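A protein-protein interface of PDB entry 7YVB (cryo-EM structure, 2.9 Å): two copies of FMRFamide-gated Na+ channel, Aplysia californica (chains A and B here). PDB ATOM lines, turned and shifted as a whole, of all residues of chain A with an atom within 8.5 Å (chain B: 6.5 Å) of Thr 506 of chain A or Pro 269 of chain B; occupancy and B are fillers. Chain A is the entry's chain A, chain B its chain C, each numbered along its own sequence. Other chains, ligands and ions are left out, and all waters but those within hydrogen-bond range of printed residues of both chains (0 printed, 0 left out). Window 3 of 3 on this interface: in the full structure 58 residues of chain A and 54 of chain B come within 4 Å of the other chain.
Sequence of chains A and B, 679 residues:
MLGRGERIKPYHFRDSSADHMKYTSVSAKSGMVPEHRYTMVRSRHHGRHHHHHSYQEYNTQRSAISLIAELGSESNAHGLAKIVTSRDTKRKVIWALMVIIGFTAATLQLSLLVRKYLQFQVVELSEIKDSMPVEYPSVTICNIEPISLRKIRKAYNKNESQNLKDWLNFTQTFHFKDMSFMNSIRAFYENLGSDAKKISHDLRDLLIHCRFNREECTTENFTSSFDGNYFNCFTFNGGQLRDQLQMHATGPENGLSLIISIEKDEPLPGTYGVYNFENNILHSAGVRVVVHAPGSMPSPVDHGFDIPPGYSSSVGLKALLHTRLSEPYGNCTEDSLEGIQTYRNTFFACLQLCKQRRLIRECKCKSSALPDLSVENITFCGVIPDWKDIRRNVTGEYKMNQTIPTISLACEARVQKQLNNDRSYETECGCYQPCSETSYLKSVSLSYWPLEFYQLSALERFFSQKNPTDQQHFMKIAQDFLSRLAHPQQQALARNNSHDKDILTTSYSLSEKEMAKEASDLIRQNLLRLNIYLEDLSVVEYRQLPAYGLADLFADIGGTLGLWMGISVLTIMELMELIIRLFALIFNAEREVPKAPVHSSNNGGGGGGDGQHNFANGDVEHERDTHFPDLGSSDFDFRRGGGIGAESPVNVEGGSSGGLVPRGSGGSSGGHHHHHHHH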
ATOM      1  N   PHE A 453     -12.697   5.517 -13.283  1.00  0.00           N
ATOM      2  CA  PHE A 453     -13.661   5.723 -12.210  1.00  0.00           C
ATOM      3  C   PHE A 453     -12.975   5.781 -10.851  1.00  0.00           C
ATOM      4  O   PHE A 453     -13.316   6.617 -10.008  1.00  0.00           O
ATOM      5  CB  PHE A 453     -14.701   4.605 -12.245  1.00  0.00           C
ATOM      6  CG  PHE A 453     -15.963   4.925 -11.512  1.00  0.00           C
ATOM      7  CD1 PHE A 453     -16.484   6.200 -11.528  1.00  0.00           C
ATOM      8  CD2 PHE A 453     -16.634   3.942 -10.810  1.00  0.00           C
ATOM      9  CE1 PHE A 453     -17.648   6.490 -10.856  1.00  0.00           C
ATOM     10  CE2 PHE A 453     -17.796   4.228 -10.138  1.00  0.00           C
ATOM     11  CZ  PHE A 453     -18.303   5.503 -10.160  1.00  0.00           C
ATOM     12  N   LEU A 482      -8.282  15.251 -11.472  1.00  0.00           N
ATOM     13  CA  LEU A 482      -9.380  14.392 -11.052  1.00  0.00           C
ATOM     14  C   LEU A 482     -10.263  15.077 -10.015  1.00  0.00           C
ATOM     15  O   LEU A 482     -11.490  14.924 -10.044  1.00  0.00           O
ATOM     16  CB  LEU A 482      -8.830  13.074 -10.523  1.00  0.00           C
ATOM     17  CG  LEU A 482      -8.212  12.232 -11.634  1.00  0.00           C
ATOM     18  CD1 LEU A 482      -7.649  10.946 -11.081  1.00  0.00           C
ATOM     19  CD2 LEU A 482      -9.241  11.952 -12.705  1.00  0.00           C
ATOM     20  N   SER A 483      -9.665  15.844  -9.103  1.00  0.00           N
ATOM     21  CA  SER A 483     -10.446  16.514  -8.075  1.00  0.00           C
ATOM     22  C   SER A 483     -11.265  17.658  -8.648  1.00  0.00           C
ATOM     23  O   SER A 483     -12.363  17.934  -8.156  1.00  0.00           O
ATOM     24  CB  SER A 483      -9.530  17.022  -6.965  1.00  0.00           C
ATOM     25  OG  SER A 483      -8.593  17.950  -7.475  1.00  0.00           O
ATOM     26  N   ARG A 484     -10.758  18.347  -9.670  1.00  0.00           N
ATOM     27  CA  ARG A 484     -11.609  19.343 -10.304  1.00  0.00           C
ATOM     28  C   ARG A 484     -12.684  18.710 -11.172  1.00  0.00           C
ATOM     29  O   ARG A 484     -13.720  19.339 -11.406  1.00  0.00           O
ATOM     30  CB  ARG A 484     -10.792  20.341 -11.128  1.00  0.00           C
ATOM     31  CG  ARG A 484      -9.841  21.178 -10.295  1.00  0.00           C
ATOM     32  CD  ARG A 484      -9.227  22.304 -11.102  1.00  0.00           C
ATOM     33  NE  ARG A 484      -8.234  21.866 -12.073  1.00  0.00           N
ATOM     34  CZ  ARG A 484      -8.472  21.753 -13.373  1.00  0.00           C
ATOM     35  NH1 ARG A 484      -9.676  22.030 -13.853  1.00  0.00           N
ATOM     36  NH2 ARG A 484      -7.513  21.355 -14.193  1.00  0.00           N
ATOM     37  N   LEU A 485     -12.467  17.485 -11.649  1.00  0.00           N
ATOM     38  CA  LEU A 485     -13.552  16.766 -12.308  1.00  0.00           C
ATOM     39  C   LEU A 485     -14.646  16.373 -11.325  1.00  0.00           C
ATOM     40  O   LEU A 485     -15.834  16.553 -11.609  1.00  0.00           O
ATOM     41  CB  LEU A 485     -13.024  15.519 -13.004  1.00  0.00           C
ATOM     42  CG  LEU A 485     -12.245  15.710 -14.294  1.00  0.00           C
ATOM     43  CD1 LEU A 485     -11.678  14.381 -14.710  1.00  0.00           C
ATOM     44  CD2 LEU A 485     -13.150  16.268 -15.365  1.00  0.00           C
ATOM     45  N   ALA A 486     -14.267  15.833 -10.169  1.00  0.00           N
ATOM     46  CA  ALA A 486     -15.240  15.319  -9.218  1.00  0.00           C
ATOM     47  C   ALA A 486     -15.885  16.402  -8.369  1.00  0.00           C
ATOM     48  O   ALA A 486     -16.884  16.125  -7.698  1.00  0.00           O
ATOM     49  CB  ALA A 486     -14.589  14.284  -8.302  1.00  0.00           C
ATOM     50  N   HIS A 487     -15.347  17.618  -8.373  1.00  0.00           N
ATOM     51  CA  HIS A 487     -15.906  18.736  -7.615  1.00  0.00           C
ATOM     52  C   HIS A 487     -16.012  19.951  -8.524  1.00  0.00           C
ATOM     53  O   HIS A 487     -15.282  20.935  -8.357  1.00  0.00           O
ATOM     54  CB  HIS A 487     -15.052  19.041  -6.385  1.00  0.00           C
ATOM     55  CG  HIS A 487     -14.717  17.833  -5.568  1.00  0.00           C
ATOM     56  ND1 HIS A 487     -15.646  16.861  -5.261  1.00  0.00           N
ATOM     57  CD2 HIS A 487     -13.556  17.437  -4.996  1.00  0.00           C
ATOM     58  CE1 HIS A 487     -15.070  15.920  -4.535  1.00  0.00           C
ATOM     59  NE2 HIS A 487     -13.802  16.245  -4.360  1.00  0.00           N
ATOM     60  N   PRO A 488     -16.910  19.911  -9.511  1.00  0.00           N
ATOM     61  CA  PRO A 488     -17.073  21.079 -10.390  1.00  0.00           C
ATOM     62  C   PRO A 488     -17.554  22.318  -9.658  1.00  0.00           C
ATOM     63  O   PRO A 488     -17.175  23.435 -10.036  1.00  0.00           O
ATOM     64  CB  PRO A 488     -18.099  20.602 -11.429  1.00  0.00           C
ATOM     65  CG  PRO A 488     -18.197  19.115 -11.252  1.00  0.00           C
ATOM     66  CD  PRO A 488     -17.886  18.856  -9.820  1.00  0.00           C
ATOM     67  N   GLN A 489     -18.372  22.150  -8.621  1.00  0.00           N
ATOM     68  CA  GLN A 489     -18.933  23.261  -7.855  1.00  0.00           C
ATOM     69  C   GLN A 489     -19.657  24.263  -8.751  1.00  0.00           C
ATOM     70  O   GLN A 489     -20.865  24.163  -8.963  1.00  0.00           O
ATOM     71  CB  GLN A 489     -17.840  23.971  -7.053  1.00  0.00           C
ATOM     72  CG  GLN A 489     -18.367  25.007  -6.077  1.00  0.00           C
ATOM     73  CD  GLN A 489     -17.303  25.500  -5.117  1.00  0.00           C
ATOM     74  OE1 GLN A 489     -16.123  25.179  -5.262  1.00  0.00           O
ATOM     75  NE2 GLN A 489     -17.716  26.284  -4.129  1.00  0.00           N
ATOM     76  N   THR A 506     -25.368  14.764 -16.684  1.00  0.00           N
ATOM     77  CA  THR A 506     -24.974  15.332 -17.965  1.00  0.00           C
ATOM     78  C   THR A 506     -23.864  14.517 -18.606  1.00  0.00           C
ATOM     79  O   THR A 506     -23.828  13.294 -18.472  1.00  0.00           O
ATOM     80  CB  THR A 506     -24.496  16.786 -17.812  1.00  0.00           C
ATOM     81  OG1 THR A 506     -23.323  16.820 -16.990  1.00  0.00           O
ATOM     82  CG2 THR A 506     -25.582  17.639 -17.175  1.00  0.00           C
ATOM     83  N   SER A 507     -22.947  15.188 -19.292  1.00  0.00           N
ATOM     84  CA  SER A 507     -21.835  14.491 -19.928  1.00  0.00           C
ATOM     85  C   SER A 507     -20.550  15.296 -19.824  1.00  0.00           C
ATOM     86  O   SER A 507     -20.582  16.524 -19.759  1.00  0.00           O
ATOM     87  CB  SER A 507     -22.153  14.206 -21.395  1.00  0.00           C
ATOM     88  OG  SER A 507     -22.375  15.409 -22.108  1.00  0.00           O
ATOM     89  N   TYR A 508     -19.418  14.605 -19.811  1.00  0.00           N
ATOM     90  CA  TYR A 508     -18.134  15.286 -19.714  1.00  0.00           C
ATOM     91  C   TYR A 508     -17.918  16.229 -20.878  1.00  0.00           C
ATOM     92  O   TYR A 508     -18.153  15.863 -22.029  1.00  0.00           O
ATOM     93  CB  TYR A 508     -16.996  14.270 -19.668  1.00  0.00           C
ATOM     94  CG  TYR A 508     -16.434  14.042 -18.289  1.00  0.00           C
ATOM     95  CD1 TYR A 508     -17.264  14.006 -17.178  1.00  0.00           C
ATOM     96  CD2 TYR A 508     -15.073  13.852 -18.098  1.00  0.00           C
ATOM     97  CE1 TYR A 508     -16.753  13.796 -15.914  1.00  0.00           C
ATOM     98  CE2 TYR A 508     -14.553  13.637 -16.838  1.00  0.00           C
ATOM     99  CZ  TYR A 508     -15.398  13.611 -15.749  1.00  0.00           C
ATOM    100  OH  TYR A 508     -14.889  13.399 -14.490  1.00  0.00           O
ATOM    101  N   SER A 509     -17.466  17.442 -20.589  1.00  0.00           N
ATOM    102  CA  SER A 509     -17.168  18.384 -21.654  1.00  0.00           C
ATOM    103  C   SER A 509     -15.870  17.959 -22.313  1.00  0.00           C
ATOM    104  O   SER A 509     -15.145  17.124 -21.779  1.00  0.00           O
ATOM    105  CB  SER A 509     -17.035  19.800 -21.108  1.00  0.00           C
ATOM    106  OG  SER A 509     -15.839  19.948 -20.365  1.00  0.00           O
ATOM    107  N   GLU A 512     -13.318  18.680 -19.883  1.00  0.00           N
ATOM    108  CA  GLU A 512     -13.439  17.691 -18.826  1.00  0.00           C
ATOM    109  C   GLU A 512     -12.875  16.380 -19.322  1.00  0.00           C
ATOM    110  O   GLU A 512     -12.150  15.695 -18.603  1.00  0.00           O
ATOM    111  CB  GLU A 512     -14.893  17.505 -18.409  1.00  0.00           C
ATOM    112  CG  GLU A 512     -15.458  18.655 -17.596  1.00  0.00           C
ATOM    113  CD  GLU A 512     -16.883  18.399 -17.146  1.00  0.00           C
ATOM    114  OE1 GLU A 512     -17.438  17.339 -17.503  1.00  0.00           O
ATOM    115  OE2 GLU A 512     -17.446  19.258 -16.435  1.00  0.00           O
ATOM    116  N   ARG B 153     -26.029   5.610 -14.942  1.00  0.00           N
ATOM    117  CA  ARG B 153     -26.426   6.932 -15.411  1.00  0.00           C
ATOM    118  C   ARG B 153     -27.867   6.933 -15.895  1.00  0.00           C
ATOM    119  O   ARG B 153     -28.622   7.875 -15.625  1.00  0.00           O
ATOM    120  CB  ARG B 153     -25.487   7.390 -16.524  1.00  0.00           C
ATOM    121  CG  ARG B 153     -25.747   8.797 -17.022  1.00  0.00           C
ATOM    122  CD  ARG B 153     -24.466   9.459 -17.509  1.00  0.00           C
ATOM    123  NE  ARG B 153     -23.524   8.494 -18.066  1.00  0.00           N
ATOM    124  CZ  ARG B 153     -23.616   7.979 -19.287  1.00  0.00           C
ATOM    125  NH1 ARG B 153     -24.612   8.334 -20.083  1.00  0.00           N
ATOM    126  NH2 ARG B 153     -22.714   7.108 -19.710  1.00  0.00           N
ATOM    127  N   ASN B 157     -30.935   9.243 -14.471  1.00  0.00           N
ATOM    128  CA  ASN B 157     -31.789  10.052 -15.340  1.00  0.00           C
ATOM    129  C   ASN B 157     -33.261   9.707 -15.154  1.00  0.00           C
ATOM    130  O   ASN B 157     -34.130  10.570 -15.331  1.00  0.00           O
ATOM    131  CB  ASN B 157     -31.378   9.883 -16.801  1.00  0.00           C
ATOM    132  CG  ASN B 157     -30.162  10.715 -17.160  1.00  0.00           C
ATOM    133  OD1 ASN B 157     -29.557  11.353 -16.299  1.00  0.00           O
ATOM    134  ND2 ASN B 157     -29.804  10.718 -18.438  1.00  0.00           N
ATOM    135  N   GLU B 266     -17.824   6.404 -19.481  1.00  0.00           N
ATOM    136  CA  GLU B 266     -17.398   7.475 -18.599  1.00  0.00           C
ATOM    137  C   GLU B 266     -18.441   7.696 -17.507  1.00  0.00           C
ATOM    138  O   GLU B 266     -19.646   7.580 -17.762  1.00  0.00           O
ATOM    139  CB  GLU B 266     -17.161   8.760 -19.391  1.00  0.00           C
ATOM    140  CG  GLU B 266     -18.401   9.359 -20.013  1.00  0.00           C
ATOM    141  CD  GLU B 266     -18.086  10.590 -20.829  1.00  0.00           C
ATOM    142  OE1 GLU B 266     -16.894  10.806 -21.133  1.00  0.00           O
ATOM    143  OE2 GLU B 266     -19.022  11.340 -21.172  1.00  0.00           O
ATOM    144  N   PRO B 267     -18.021   7.999 -16.286  1.00  0.00           N
ATOM    145  CA  PRO B 267     -18.975   8.095 -15.175  1.00  0.00           C
ATOM    146  C   PRO B 267     -19.841   9.339 -15.234  1.00  0.00           C
ATOM    147  O   PRO B 267     -19.790  10.101 -16.204  1.00  0.00           O
ATOM    148  CB  PRO B 267     -18.066   8.118 -13.942  1.00  0.00           C
ATOM    149  CG  PRO B 267     -16.787   8.685 -14.441  1.00  0.00           C
ATOM    150  CD  PRO B 267     -16.630   8.165 -15.836  1.00  0.00           C
ATOM    151  N   LEU B 268     -20.642   9.547 -14.193  1.00  0.00           N
ATOM    152  CA  LEU B 268     -21.442  10.749 -14.094  1.00  0.00           C
ATOM    153  C   LEU B 268     -20.531  11.965 -13.951  1.00  0.00           C
ATOM    154  O   LEU B 268     -19.385  11.843 -13.511  1.00  0.00           O
ATOM    155  CB  LEU B 268     -22.399  10.652 -12.911  1.00  0.00           C
ATOM    156  CG  LEU B 268     -23.738   9.975 -13.206  1.00  0.00           C
ATOM    157  CD1 LEU B 268     -23.582   8.466 -13.206  1.00  0.00           C
ATOM    158  CD2 LEU B 268     -24.794  10.407 -12.205  1.00  0.00           C
ATOM    159  N   PRO B 269     -21.016  13.149 -14.330  1.00  0.00           N
ATOM    160  CA  PRO B 269     -20.133  14.328 -14.372  1.00  0.00           C
ATOM    161  C   PRO B 269     -19.399  14.620 -13.072  1.00  0.00           C
ATOM    162  O   PRO B 269     -18.242  15.053 -13.114  1.00  0.00           O
ATOM    163  CB  PRO B 269     -21.089  15.473 -14.733  1.00  0.00           C
ATOM    164  CG  PRO B 269     -22.422  14.850 -15.034  1.00  0.00           C
ATOM    165  CD  PRO B 269     -22.278  13.373 -15.049  1.00  0.00           C
ATOM    166  N   GLY B 270     -20.028  14.400 -11.922  1.00  0.00           N
ATOM    167  CA  GLY B 270     -19.375  14.703 -10.665  1.00  0.00           C
ATOM    168  C   GLY B 270     -19.270  13.513  -9.739  1.00  0.00           C
ATOM    169  O   GLY B 270     -19.437  13.646  -8.523  1.00  0.00           O
ATOM    170  N   THR B 271     -18.989  12.344 -10.299  1.00  0.00           N
ATOM    171  CA  THR B 271     -19.003  11.096  -9.552  1.00  0.00           C
ATOM    172  C   THR B 271     -17.690  10.357  -9.753  1.00  0.00           C
ATOM    173  O   THR B 271     -17.160  10.308 -10.865  1.00  0.00           O
ATOM    174  CB  THR B 271     -20.178  10.219  -9.995  1.00  0.00           C
ATOM    175  OG1 THR B 271     -21.396  10.749  -9.459  1.00  0.00           O
ATOM    176  CG2 THR B 271     -20.004   8.795  -9.527  1.00  0.00           C
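O of Pro 269 of chain B lies close to O of Leu 485 of chain A (3.2 Å).
Among the printed residues, pairs that only touch across the chains: Phe 453 of chain A with Pro 267 of chain B, Phe 453 of chain A with Thr 271 of chain B, Ala 486 of chain A with Gly 270 of chain B, Thr 506 of chain A with Pro 269 of chain B, Tyr 508 of chain A with Glu 266 of chain B and Tyr 508 of chain A with Pro 269 of chain B.
Of the printed residues of chain B, Thr 506 of chain A touches Pro 269 (2.9 Å). Printed residues of chain A within 4 Å of Pro 269 of chain B: Leu 485 (3.2 Å), Thr 506 (2.9 Å) and Tyr 508 (3.4 Å). Printed residues of chain A within 4 Å of Pro 267 of chain B: Phe 453. Of the printed residues of chain A, Glu 266 of chain B touches Tyr 508. Printed residues of chain B within 4 Å of Leu 485 of chain A: Pro 269 (3.2 Å). Of the printed residues of chain A, Thr 271 of chain B touches Phe 453. Arg 484 of chain A touches none of the printed residues of chain B. Leu 268 of chain B touches none of the printed residues of chain A. The nearest printed residue of chain A that does not touch Pro 267 of chain B is Tyr 508 of chain A (4.8 Å).
Of the 14 printed residues of chain A, 5 touch a printed residue of chain B. Hydrophobic or aromatic side chains of chain A within 4 Å of the printed part of chain B: Phe 453 and Tyr 508. Of the 8 printed residues of chain B, 5 touch a printed residue of chain A. Hydrophobic or aromatic side chains of chain B that line the printed part of chain A: Pro 267 and Pro 269.
No position is printed for both chains. Of the 7 pairs that touch across the chains among the printed residues, none has its exchanged pair printed and touching as well.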
